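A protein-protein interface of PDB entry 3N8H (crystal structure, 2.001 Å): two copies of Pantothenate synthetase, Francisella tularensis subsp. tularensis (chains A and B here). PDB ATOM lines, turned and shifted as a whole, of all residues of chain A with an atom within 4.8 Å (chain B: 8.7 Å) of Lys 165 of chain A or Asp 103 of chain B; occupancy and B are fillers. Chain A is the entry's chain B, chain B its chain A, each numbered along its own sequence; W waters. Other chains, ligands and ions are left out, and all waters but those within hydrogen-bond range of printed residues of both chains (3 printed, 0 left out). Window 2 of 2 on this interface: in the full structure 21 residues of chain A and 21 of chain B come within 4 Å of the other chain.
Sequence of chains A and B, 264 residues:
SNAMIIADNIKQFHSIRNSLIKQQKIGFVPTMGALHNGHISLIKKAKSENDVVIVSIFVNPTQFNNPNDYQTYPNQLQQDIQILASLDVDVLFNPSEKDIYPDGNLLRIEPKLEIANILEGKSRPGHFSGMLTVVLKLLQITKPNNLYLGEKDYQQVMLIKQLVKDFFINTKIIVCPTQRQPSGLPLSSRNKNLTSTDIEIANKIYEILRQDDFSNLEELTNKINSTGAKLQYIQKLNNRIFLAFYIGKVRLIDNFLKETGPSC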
ATOM      1  N   LYS A 161       1.721  -8.840  11.186  1.00  0.00           N
ATOM      2  CA  LYS A 161       3.016  -8.294  11.564  1.00  0.00           C
ATOM      3  C   LYS A 161       4.128  -9.121  10.920  1.00  0.00           C
ATOM      4  O   LYS A 161       5.115  -8.565  10.424  1.00  0.00           O
ATOM      5  CB  LYS A 161       3.190  -8.275  13.094  1.00  0.00           C
ATOM      6  CG  LYS A 161       2.364  -7.211  13.787  1.00  0.00           C
ATOM      7  CD  LYS A 161       2.496  -7.259  15.309  1.00  0.00           C
ATOM      8  CE  LYS A 161       1.862  -6.003  15.928  1.00  0.00           C
ATOM      9  NZ  LYS A 161       2.082  -5.899  17.400  1.00  0.00           N
ATOM     10  N   GLN A 162       3.975 -10.446  10.931  1.00  0.00           N
ATOM     11  CA  GLN A 162       5.029 -11.324  10.394  1.00  0.00           C
ATOM     12  C   GLN A 162       5.073 -11.133   8.893  1.00  0.00           C
ATOM     13  O   GLN A 162       6.137 -11.027   8.289  1.00  0.00           O
ATOM     14  CB  GLN A 162       4.759 -12.793  10.725  1.00  0.00           C
ATOM     15  CG  GLN A 162       5.893 -13.733  10.305  1.00  0.00           C
ATOM     16  CD  GLN A 162       7.130 -13.561  11.172  1.00  0.00           C
ATOM     17  OE1 GLN A 162       7.036 -13.502  12.403  1.00  0.00           O
ATOM     18  NE2 GLN A 162       8.297 -13.486  10.536  1.00  0.00           N
ATOM     19  N   LEU A 163       3.890 -11.061   8.298  1.00  0.00           N
ATOM     20  CA  LEU A 163       3.779 -10.807   6.869  1.00  0.00           C
ATOM     21  C   LEU A 163       4.506  -9.519   6.446  1.00  0.00           C
ATOM     22  O   LEU A 163       5.266  -9.514   5.492  1.00  0.00           O
ATOM     23  CB  LEU A 163       2.301 -10.737   6.459  1.00  0.00           C
ATOM     24  CG  LEU A 163       2.032 -10.446   4.985  1.00  0.00           C
ATOM     25  CD1 LEU A 163       2.086 -11.724   4.134  1.00  0.00           C
ATOM     26  CD2 LEU A 163       0.679  -9.709   4.822  1.00  0.00           C
ATOM     27  N   VAL A 164       4.248  -8.420   7.131  1.00  0.00           N
ATOM     28  CA  VAL A 164       4.871  -7.141   6.758  1.00  0.00           C
ATOM     29  C   VAL A 164       6.389  -7.215   6.946  1.00  0.00           C
ATOM     30  O   VAL A 164       7.159  -6.690   6.156  1.00  0.00           O
ATOM     31  CB  VAL A 164       4.231  -5.966   7.583  1.00  0.00           C
ATOM     32  CG1 VAL A 164       5.162  -4.765   7.685  1.00  0.00           C
ATOM     33  CG2 VAL A 164       2.894  -5.576   6.965  1.00  0.00           C
ATOM     34  N   LYS A 165       6.808  -7.896   7.997  1.00  0.00           N
ATOM     35  CA  LYS A 165       8.232  -8.119   8.238  1.00  0.00           C
ATOM     36  C   LYS A 165       8.871  -8.945   7.122  1.00  0.00           C
ATOM     37  O   LYS A 165       9.897  -8.543   6.563  1.00  0.00           O
ATOM     38  CB  LYS A 165       8.434  -8.798   9.594  1.00  0.00           C
ATOM     39  CG  LYS A 165       9.875  -9.087   9.992  1.00  0.00           C
ATOM     40  CD  LYS A 165       9.913  -9.699  11.397  1.00  0.00           C
ATOM     41  CE  LYS A 165      11.356  -9.787  11.906  1.00  0.00           C
ATOM     42  NZ  LYS A 165      11.572 -10.670  13.111  1.00  0.00           N
ATOM     43  N   ASP A 166       8.272 -10.089   6.794  1.00  0.00           N
ATOM     44  CA  ASP A 166       8.900 -11.052   5.866  1.00  0.00           C
ATOM     45  C   ASP A 166       8.924 -10.590   4.428  1.00  0.00           C
ATOM     46  O   ASP A 166       9.827 -10.959   3.679  1.00  0.00           O
ATOM     47  CB  ASP A 166       8.217 -12.414   5.921  1.00  0.00           C
ATOM     48  CG  ASP A 166       8.854 -13.351   6.936  1.00  0.00           C
ATOM     49  OD1 ASP A 166      10.096 -13.511   6.914  1.00  0.00           O
ATOM     50  OD2 ASP A 166       8.104 -13.948   7.735  1.00  0.00           O
ATOM     51  N   PHE A 167       7.933  -9.791   4.029  1.00  0.00           N
ATOM     52  CA  PHE A 167       7.915  -9.320   2.641  1.00  0.00           C
ATOM     53  C   PHE A 167       8.299  -7.872   2.479  1.00  0.00           C
ATOM     54  O   PHE A 167       7.987  -7.244   1.466  1.00  0.00           O
ATOM     55  CB  PHE A 167       6.616  -9.737   1.922  1.00  0.00           C
ATOM     56  CG  PHE A 167       6.468 -11.235   1.871  1.00  0.00           C
ATOM     57  CD1 PHE A 167       7.336 -11.986   1.080  1.00  0.00           C
ATOM     58  CD2 PHE A 167       5.551 -11.901   2.687  1.00  0.00           C
ATOM     59  CE1 PHE A 167       7.272 -13.376   1.066  1.00  0.00           C
ATOM     60  CE2 PHE A 167       5.468 -13.298   2.671  1.00  0.00           C
ATOM     61  CZ  PHE A 167       6.326 -14.032   1.850  1.00  0.00           C
ATOM     62  N   PHE A 168       9.007  -7.368   3.488  1.00  0.00           N
ATOM     63  CA  PHE A 168       9.659  -6.069   3.430  1.00  0.00           C
ATOM     64  C   PHE A 168       8.689  -4.974   2.987  1.00  0.00           C
ATOM     65  O   PHE A 168       8.964  -4.196   2.074  1.00  0.00           O
ATOM     66  CB  PHE A 168      10.928  -6.161   2.563  1.00  0.00           C
ATOM     67  CG  PHE A 168      11.840  -7.289   2.994  1.00  0.00           C
ATOM     68  CD1 PHE A 168      12.781  -7.097   4.002  1.00  0.00           C
ATOM     69  CD2 PHE A 168      11.711  -8.561   2.437  1.00  0.00           C
ATOM     70  CE1 PHE A 168      13.587  -8.155   4.432  1.00  0.00           C
ATOM     71  CE2 PHE A 168      12.509  -9.630   2.880  1.00  0.00           C
ATOM     72  CZ  PHE A 168      13.449  -9.419   3.870  1.00  0.00           C
ATOM     73  N   ILE B  10      20.695  -6.172   4.244  1.00  0.00           N
ATOM     74  CA  ILE B  10      19.543  -5.334   3.921  1.00  0.00           C
ATOM     75  C   ILE B  10      19.782  -3.843   4.171  1.00  0.00           C
ATOM     76  O   ILE B  10      19.579  -3.011   3.273  1.00  0.00           O
ATOM     77  CB  ILE B  10      18.283  -5.781   4.715  1.00  0.00           C
ATOM     78  CG1 ILE B  10      18.028  -7.273   4.515  1.00  0.00           C
ATOM     79  CG2 ILE B  10      17.059  -4.991   4.278  1.00  0.00           C
ATOM     80  CD1 ILE B  10      17.706  -7.633   3.094  1.00  0.00           C
ATOM     81  N   HIS B  14      19.379  -1.183   1.449  1.00  0.00           N
ATOM     82  CA  HIS B  14      18.396  -0.102   1.493  1.00  0.00           C
ATOM     83  C   HIS B  14      19.080   1.227   1.280  1.00  0.00           C
ATOM     84  O   HIS B  14      18.576   2.082   0.552  1.00  0.00           O
ATOM     85  CB  HIS B  14      17.642  -0.088   2.809  1.00  0.00           C
ATOM     86  CG  HIS B  14      16.629  -1.180   2.930  1.00  0.00           C
ATOM     87  ND1 HIS B  14      15.800  -1.541   1.889  1.00  0.00           N
ATOM     88  CD2 HIS B  14      16.300  -1.980   3.970  1.00  0.00           C
ATOM     89  CE1 HIS B  14      15.010  -2.526   2.280  1.00  0.00           C
ATOM     90  NE2 HIS B  14      15.293  -2.811   3.538  1.00  0.00           N
ATOM     91  N   GLU B  97      21.357 -15.948   4.865  1.00  0.00           N
ATOM     92  CA  GLU B  97      20.089 -16.593   5.172  1.00  0.00           C
ATOM     93  C   GLU B  97      19.292 -15.770   6.169  1.00  0.00           C
ATOM     94  O   GLU B  97      18.083 -15.608   6.025  1.00  0.00           O
ATOM     95  CB  GLU B  97      20.344 -17.959   5.792  1.00  0.00           C
ATOM     96  CG  GLU B  97      19.983 -19.128   4.927  1.00  0.00           C
ATOM     97  CD  GLU B  97      19.895 -20.401   5.740  1.00  0.00           C
ATOM     98  OE1 GLU B  97      20.876 -21.170   5.753  1.00  0.00           O
ATOM     99  OE2 GLU B  97      18.844 -20.623   6.371  1.00  0.00           O
ATOM    100  N   LYS B  98      19.975 -15.272   7.197  1.00  0.00           N
ATOM    101  CA  LYS B  98      19.317 -14.525   8.258  1.00  0.00           C
ATOM    102  C   LYS B  98      18.729 -13.224   7.728  1.00  0.00           C
ATOM    103  O   LYS B  98      17.652 -12.811   8.144  1.00  0.00           O
ATOM    104  CB  LYS B  98      20.299 -14.220   9.388  1.00  0.00           C
ATOM    105  CG  LYS B  98      20.706 -15.412  10.233  1.00  0.00           C
ATOM    106  CD  LYS B  98      21.913 -15.067  11.124  1.00  0.00           C
ATOM    107  CE  LYS B  98      21.627 -13.872  12.034  1.00  0.00           C
ATOM    108  NZ  LYS B  98      21.475 -12.576  11.305  1.00  0.00           N
ATOM    109  N   ASP B  99      19.446 -12.565   6.822  1.00  0.00           N
ATOM    110  CA  ASP B  99      18.917 -11.345   6.200  1.00  0.00           C
ATOM    111  C   ASP B  99      17.552 -11.644   5.549  1.00  0.00           C
ATOM    112  O   ASP B  99      16.587 -10.892   5.699  1.00  0.00           O
ATOM    113  CB  ASP B  99      19.873 -10.831   5.127  1.00  0.00           C
ATOM    114  CG  ASP B  99      21.175 -10.285   5.706  1.00  0.00           C
ATOM    115  OD1 ASP B  99      22.215 -10.350   5.007  1.00  0.00           O
ATOM    116  OD2 ASP B  99      21.156  -9.811   6.860  1.00  0.00           O
ATOM    117  N   ILE B 100      17.483 -12.750   4.821  1.00  0.00           N
ATOM    118  CA  ILE B 100      16.315 -13.028   3.988  1.00  0.00           C
ATOM    119  C   ILE B 100      15.175 -13.677   4.764  1.00  0.00           C
ATOM    120  O   ILE B 100      13.985 -13.392   4.519  1.00  0.00           O
ATOM    121  CB  ILE B 100      16.690 -13.876   2.738  1.00  0.00           C
ATOM    122  CG1 ILE B 100      17.693 -13.115   1.872  1.00  0.00           C
ATOM    123  CG2 ILE B 100      15.445 -14.199   1.910  1.00  0.00           C
ATOM    124  CD1 ILE B 100      17.204 -11.734   1.422  1.00  0.00           C
ATOM    125  N   TYR B 101      15.547 -14.551   5.694  1.00  0.00           N
ATOM    126  CA  TYR B 101      14.598 -15.255   6.547  1.00  0.00           C
ATOM    127  C   TYR B 101      14.936 -14.985   7.997  1.00  0.00           C
ATOM    128  O   TYR B 101      15.484 -15.844   8.673  1.00  0.00           O
ATOM    129  CB  TYR B 101      14.707 -16.751   6.325  1.00  0.00           C
ATOM    130  CG  TYR B 101      14.405 -17.160   4.917  1.00  0.00           C
ATOM    131  CD1 TYR B 101      13.083 -17.341   4.486  1.00  0.00           C
ATOM    132  CD2 TYR B 101      15.439 -17.360   4.011  1.00  0.00           C
ATOM    133  CE1 TYR B 101      12.818 -17.721   3.192  1.00  0.00           C
ATOM    134  CE2 TYR B 101      15.190 -17.749   2.725  1.00  0.00           C
ATOM    135  CZ  TYR B 101      13.887 -17.928   2.311  1.00  0.00           C
ATOM    136  OH  TYR B 101      13.670 -18.318   1.010  1.00  0.00           O
ATOM    137  N   PRO B 102      14.608 -13.780   8.482  1.00  0.00           N
ATOM    138  CA  PRO B 102      14.920 -13.394   9.858  1.00  0.00           C
ATOM    139  C   PRO B 102      14.390 -14.389  10.893  1.00  0.00           C
ATOM    140  O   PRO B 102      15.054 -14.615  11.900  1.00  0.00           O
ATOM    141  CB  PRO B 102      14.229 -12.028  10.012  1.00  0.00           C
ATOM    142  CG  PRO B 102      13.279 -11.918   8.828  1.00  0.00           C
ATOM    143  CD  PRO B 102      13.954 -12.696   7.733  1.00  0.00           C
ATOM    144  N   ASP B 103      13.217 -14.980  10.641  1.00  0.00           N
ATOM    145  CA  ASP B 103      12.545 -15.836  11.621  1.00  0.00           C
ATOM    146  C   ASP B 103      12.373 -17.251  11.067  1.00  0.00           C
ATOM    147  O   ASP B 103      11.578 -18.044  11.576  1.00  0.00           O
ATOM    148  CB  ASP B 103      11.165 -15.257  11.985  1.00  0.00           C
ATOM    149  CG  ASP B 103      11.257 -13.856  12.569  1.00  0.00           C
ATOM    150  OD1 ASP B 103      12.000 -13.694  13.564  1.00  0.00           O
ATOM    151  OD2 ASP B 103      10.601 -12.917  12.037  1.00  0.00           O
ATOM    152  N   GLY B 104      13.132 -17.558  10.022  1.00  0.00           N
ATOM    153  CA  GLY B 104      13.009 -18.829   9.334  1.00  0.00           C
ATOM    154  C   GLY B 104      11.969 -18.769   8.233  1.00  0.00           C
ATOM    155  O   GLY B 104      11.469 -17.699   7.891  1.00  0.00           O
ATOM    156  N   ASN B 105      11.618 -19.932   7.698  1.00  0.00           N
ATOM    157  CA  ASN B 105      10.680 -20.010   6.588  1.00  0.00           C
ATOM    158  C   ASN B 105       9.258 -20.206   7.086  1.00  0.00           C
ATOM    159  O   ASN B 105       8.701 -21.285   6.960  1.00  0.00           O
ATOM    160  CB  ASN B 105      11.083 -21.147   5.627  1.00  0.00           C
ATOM    161  CG  ASN B 105      10.344 -21.091   4.299  1.00  0.00           C
ATOM    162  OD1 ASN B 105       9.928 -20.033   3.846  1.00  0.00           O
ATOM    163  ND2 ASN B 105      10.205 -22.244   3.655  1.00  0.00           N
ATOM    164  N   LEU B 106       8.669 -19.144   7.626  1.00  0.00           N
ATOM    165  CA  LEU B 106       7.405 -19.240   8.354  1.00  0.00           C
ATOM    166  C   LEU B 106       6.200 -18.935   7.461  1.00  0.00           C
ATOM    167  O   LEU B 106       5.145 -19.530   7.633  1.00  0.00           O
ATOM    168  CB  LEU B 106       7.409 -18.309   9.566  1.00  0.00           C
ATOM    169  CG  LEU B 106       8.459 -18.556  10.655  1.00  0.00           C
ATOM    170  CD1 LEU B 106       8.090 -17.752  11.865  1.00  0.00           C
ATOM    171  CD2 LEU B 106       8.593 -20.050  11.004  1.00  0.00           C
ATOM    172  N   LEU B 107       6.368 -18.003   6.524  1.00  0.00           N
ATOM    173  CA  LEU B 107       5.305 -17.646   5.561  1.00  0.00           C
ATOM    174  C   LEU B 107       5.783 -17.923   4.141  1.00  0.00           C
ATOM    175  O   LEU B 107       6.807 -17.381   3.704  1.00  0.00           O
ATOM    176  CB  LEU B 107       4.941 -16.161   5.684  1.00  0.00           C
ATOM    177  CG  LEU B 107       4.410 -15.685   7.036  1.00  0.00           C
ATOM    178  CD1 LEU B 107       4.147 -14.164   6.973  1.00  0.00           C
ATOM    179  CD2 LEU B 107       3.168 -16.456   7.442  1.00  0.00           C
ATOM    180  N   ARG B 108       5.048 -18.761   3.424  1.00  0.00           N
ATOM    181  CA  ARG B 108       5.519 -19.250   2.143  1.00  0.00           C
ATOM    182  C   ARG B 108       4.484 -19.005   1.075  1.00  0.00           C
ATOM    183  O   ARG B 108       3.283 -19.096   1.334  1.00  0.00           O
ATOM    184  CB  ARG B 108       5.779 -20.766   2.214  1.00  0.00           C
ATOM    185  CG  ARG B 108       6.848 -21.160   3.205  1.00  0.00           C
ATOM    186  CD  ARG B 108       6.589 -22.541   3.700  1.00  0.00           C
ATOM    187  NE  ARG B 108       7.293 -22.803   4.943  1.00  0.00           N
ATOM    188  CZ  ARG B 108       7.679 -24.013   5.325  1.00  0.00           C
ATOM    189  NH1 ARG B 108       7.426 -25.060   4.549  1.00  0.00           N
ATOM    190  NH2 ARG B 108       8.317 -24.176   6.474  1.00  0.00           N
ATOM    191  N   LYS B 137      10.448 -11.923  -2.045  1.00  0.00           N
ATOM    192  CA  LYS B 137      11.275 -11.141  -1.116  1.00  0.00           C
ATOM    193  C   LYS B 137      12.300 -10.247  -1.839  1.00  0.00           C
ATOM    194  O   LYS B 137      12.450  -9.058  -1.534  1.00  0.00           O
ATOM    195  CB  LYS B 137      11.992 -12.098  -0.151  1.00  0.00           C
ATOM    196  CG  LYS B 137      11.079 -12.676   0.939  1.00  0.00           C
ATOM    197  CD  LYS B 137      11.778 -13.868   1.642  1.00  0.00           C
ATOM    198  CE  LYS B 137      10.966 -14.338   2.869  1.00  0.00           C
ATOM    199  NZ  LYS B 137      11.200 -13.472   4.067  1.00  0.00           N
ATOM    200  N   GLN B 140      10.772  -7.345  -3.503  1.00  0.00           N
ATOM    201  CA  GLN B 140      10.254  -6.385  -2.528  1.00  0.00           C
ATOM    202  C   GLN B 140      11.425  -5.562  -2.011  1.00  0.00           C
ATOM    203  O   GLN B 140      11.299  -4.384  -1.704  1.00  0.00           O
ATOM    204  CB  GLN B 140       9.561  -7.116  -1.388  1.00  0.00           C
ATOM    205  CG  GLN B 140       8.180  -7.736  -1.746  1.00  0.00           C
ATOM    206  CD  GLN B 140       7.117  -6.658  -2.000  1.00  0.00           C
ATOM    207  OE1 GLN B 140       6.912  -6.222  -3.140  1.00  0.00           O
ATOM    208  NE2 GLN B 140       6.458  -6.210  -0.932  1.00  0.00           N
ATOM    209  N   ILE B 141      12.586  -6.194  -1.963  1.00  0.00           N
ATOM    210  CA  ILE B 141      13.801  -5.530  -1.527  1.00  0.00           C
ATOM    211  C   ILE B 141      14.332  -4.636  -2.648  1.00  0.00           C
ATOM    212  O   ILE B 141      14.626  -3.478  -2.418  1.00  0.00           O
ATOM    213  CB  ILE B 141      14.889  -6.565  -1.099  1.00  0.00           C
ATOM    214  CG1 ILE B 141      14.418  -7.345   0.139  1.00  0.00           C
ATOM    215  CG2 ILE B 141      16.215  -5.859  -0.814  1.00  0.00           C
ATOM    216  CD1 ILE B 141      15.206  -8.671   0.371  1.00  0.00           C
HETATM  217  O   HOH W   1       8.806 -12.570  14.955  1.00  0.00           O
HETATM  218  O   HOH W   2       8.943 -16.245   7.356  1.00  0.00           O
HETATM  219  O   HOH W   3      11.509 -15.087   8.348  1.00  0.00           O
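NE2 of Gln 162 of chain A lies within hydrogen-bond range of OD2 of Asp 103 of chain B (2.8 Å). The side-chain carboxylate (OD2) of Asp 103 of chain B is in salt-bridge range of the side-chain amino group (NZ) of Lys 165 of chain A (2.7 Å). NZ of Lys 137 of chain B is in salt-bridge range of OD1 of Asp 166 of chain A, at 3.1 Å. NE2 of Gln 140 of chain B is in hydrogen-bond range of O of Phe 167 of chain A.
Hydrophobic or aromatic side chains of chain A that line the printed part of chain B: Leu 163, Phe 167 and Phe 168. Hydrophobic or aromatic side chains of chain B that line the printed part of chain A: Leu 107 and Ile 141. Among the printed residues, 11 pairs touch across the chains. Among the printed residues, Asp or Glu carboxylates within 4 Å of a Lys or Arg side-chain nitrogen of the other chain: Lys 165 of chain A with Asp 103 of chain B (2.7 Å) and Asp 166 of chain A with Lys 137 of chain B (3.1 Å).
Lys 165 of chain A touches one residue of chain B. Asp 103 of chain B touches two residues of chain A. Printed residues of chain A within 4 Å of Gln 140 of chain B: Phe 167 (3.0 Å). Of the printed residues of chain A, Asp 99 of chain B touches Phe 168. Printed residues of chain B within 4 Å of Leu 163 of chain A: Leu 107 (3.4 Å). Leu 106 of chain B touches none of the printed residues of chain A. The nearest residue of chain B that does not touch Lys 165 of chain A is Pro 102 of chain B (4.1 Å).
The backbone carbonyl oxygen (O) of Ile 100 of chain B is in hydrogen-bond range of the side-chain amino group (NZ) of Lys 137 of chain B (2.8 Å). The side-chain amide nitrogen (NE2) of Gln 162 of chain A is in hydrogen-bond range of the side-chain carboxylate (OD2) of Asp 166 of chain A (2.8 Å).
No position is printed for both chains. Of the 11 pairs that touch across the chains among the printed residues, none has its exchanged pair printed and touching as well.
Water W2 lies within hydrogen-bond range of the side-chain carboxylate of Asp 166 of chain A (2.5 Å), the backbone NH of Leu 106 of chain B (2.9 Å), the backbone carbonyl oxygen of Gly 104 of chain B (3.0 Å) and the backbone NH of Leu 107 of chain B (3.2 Å). Water W3 lies within hydrogen-bond range of the side-chain carboxylate (OD1) of Asp 166 of chain A (2.6 Å), the backbone carbonyl oxygen (O) of Gly 104 of chain B (2.7 Å) and the backbone NH (N) of Asp 103 of chain B (2.9 Å). Water W1 bridges the side-chain amide oxygen (OE1) of Gln 162 of chain A and the side-chain carboxylate (OD2) of Asp 103 of chain B.
Gln 162 of chain A touches Leu 107 of chain B (C to CD1, 3.7 Å). Leu 163 of chain A touches Leu 107 of chain B (CA to CD1, 3.4 Å). CZ of Phe 167 of chain A touches O of Leu 107 of chain B (3.9 Å). Phe 167 of chain A touches Lys 137 of chain B (CD1 to CG, 3.8 Å). Phe 168 of chain A touches Asp 99 of chain B. CG of Lys 137 of chain B touches CE2 of Phe 168 of chain A, 3.9 Å away. Phe 168 of chain A touches Ile 141 of chain B.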
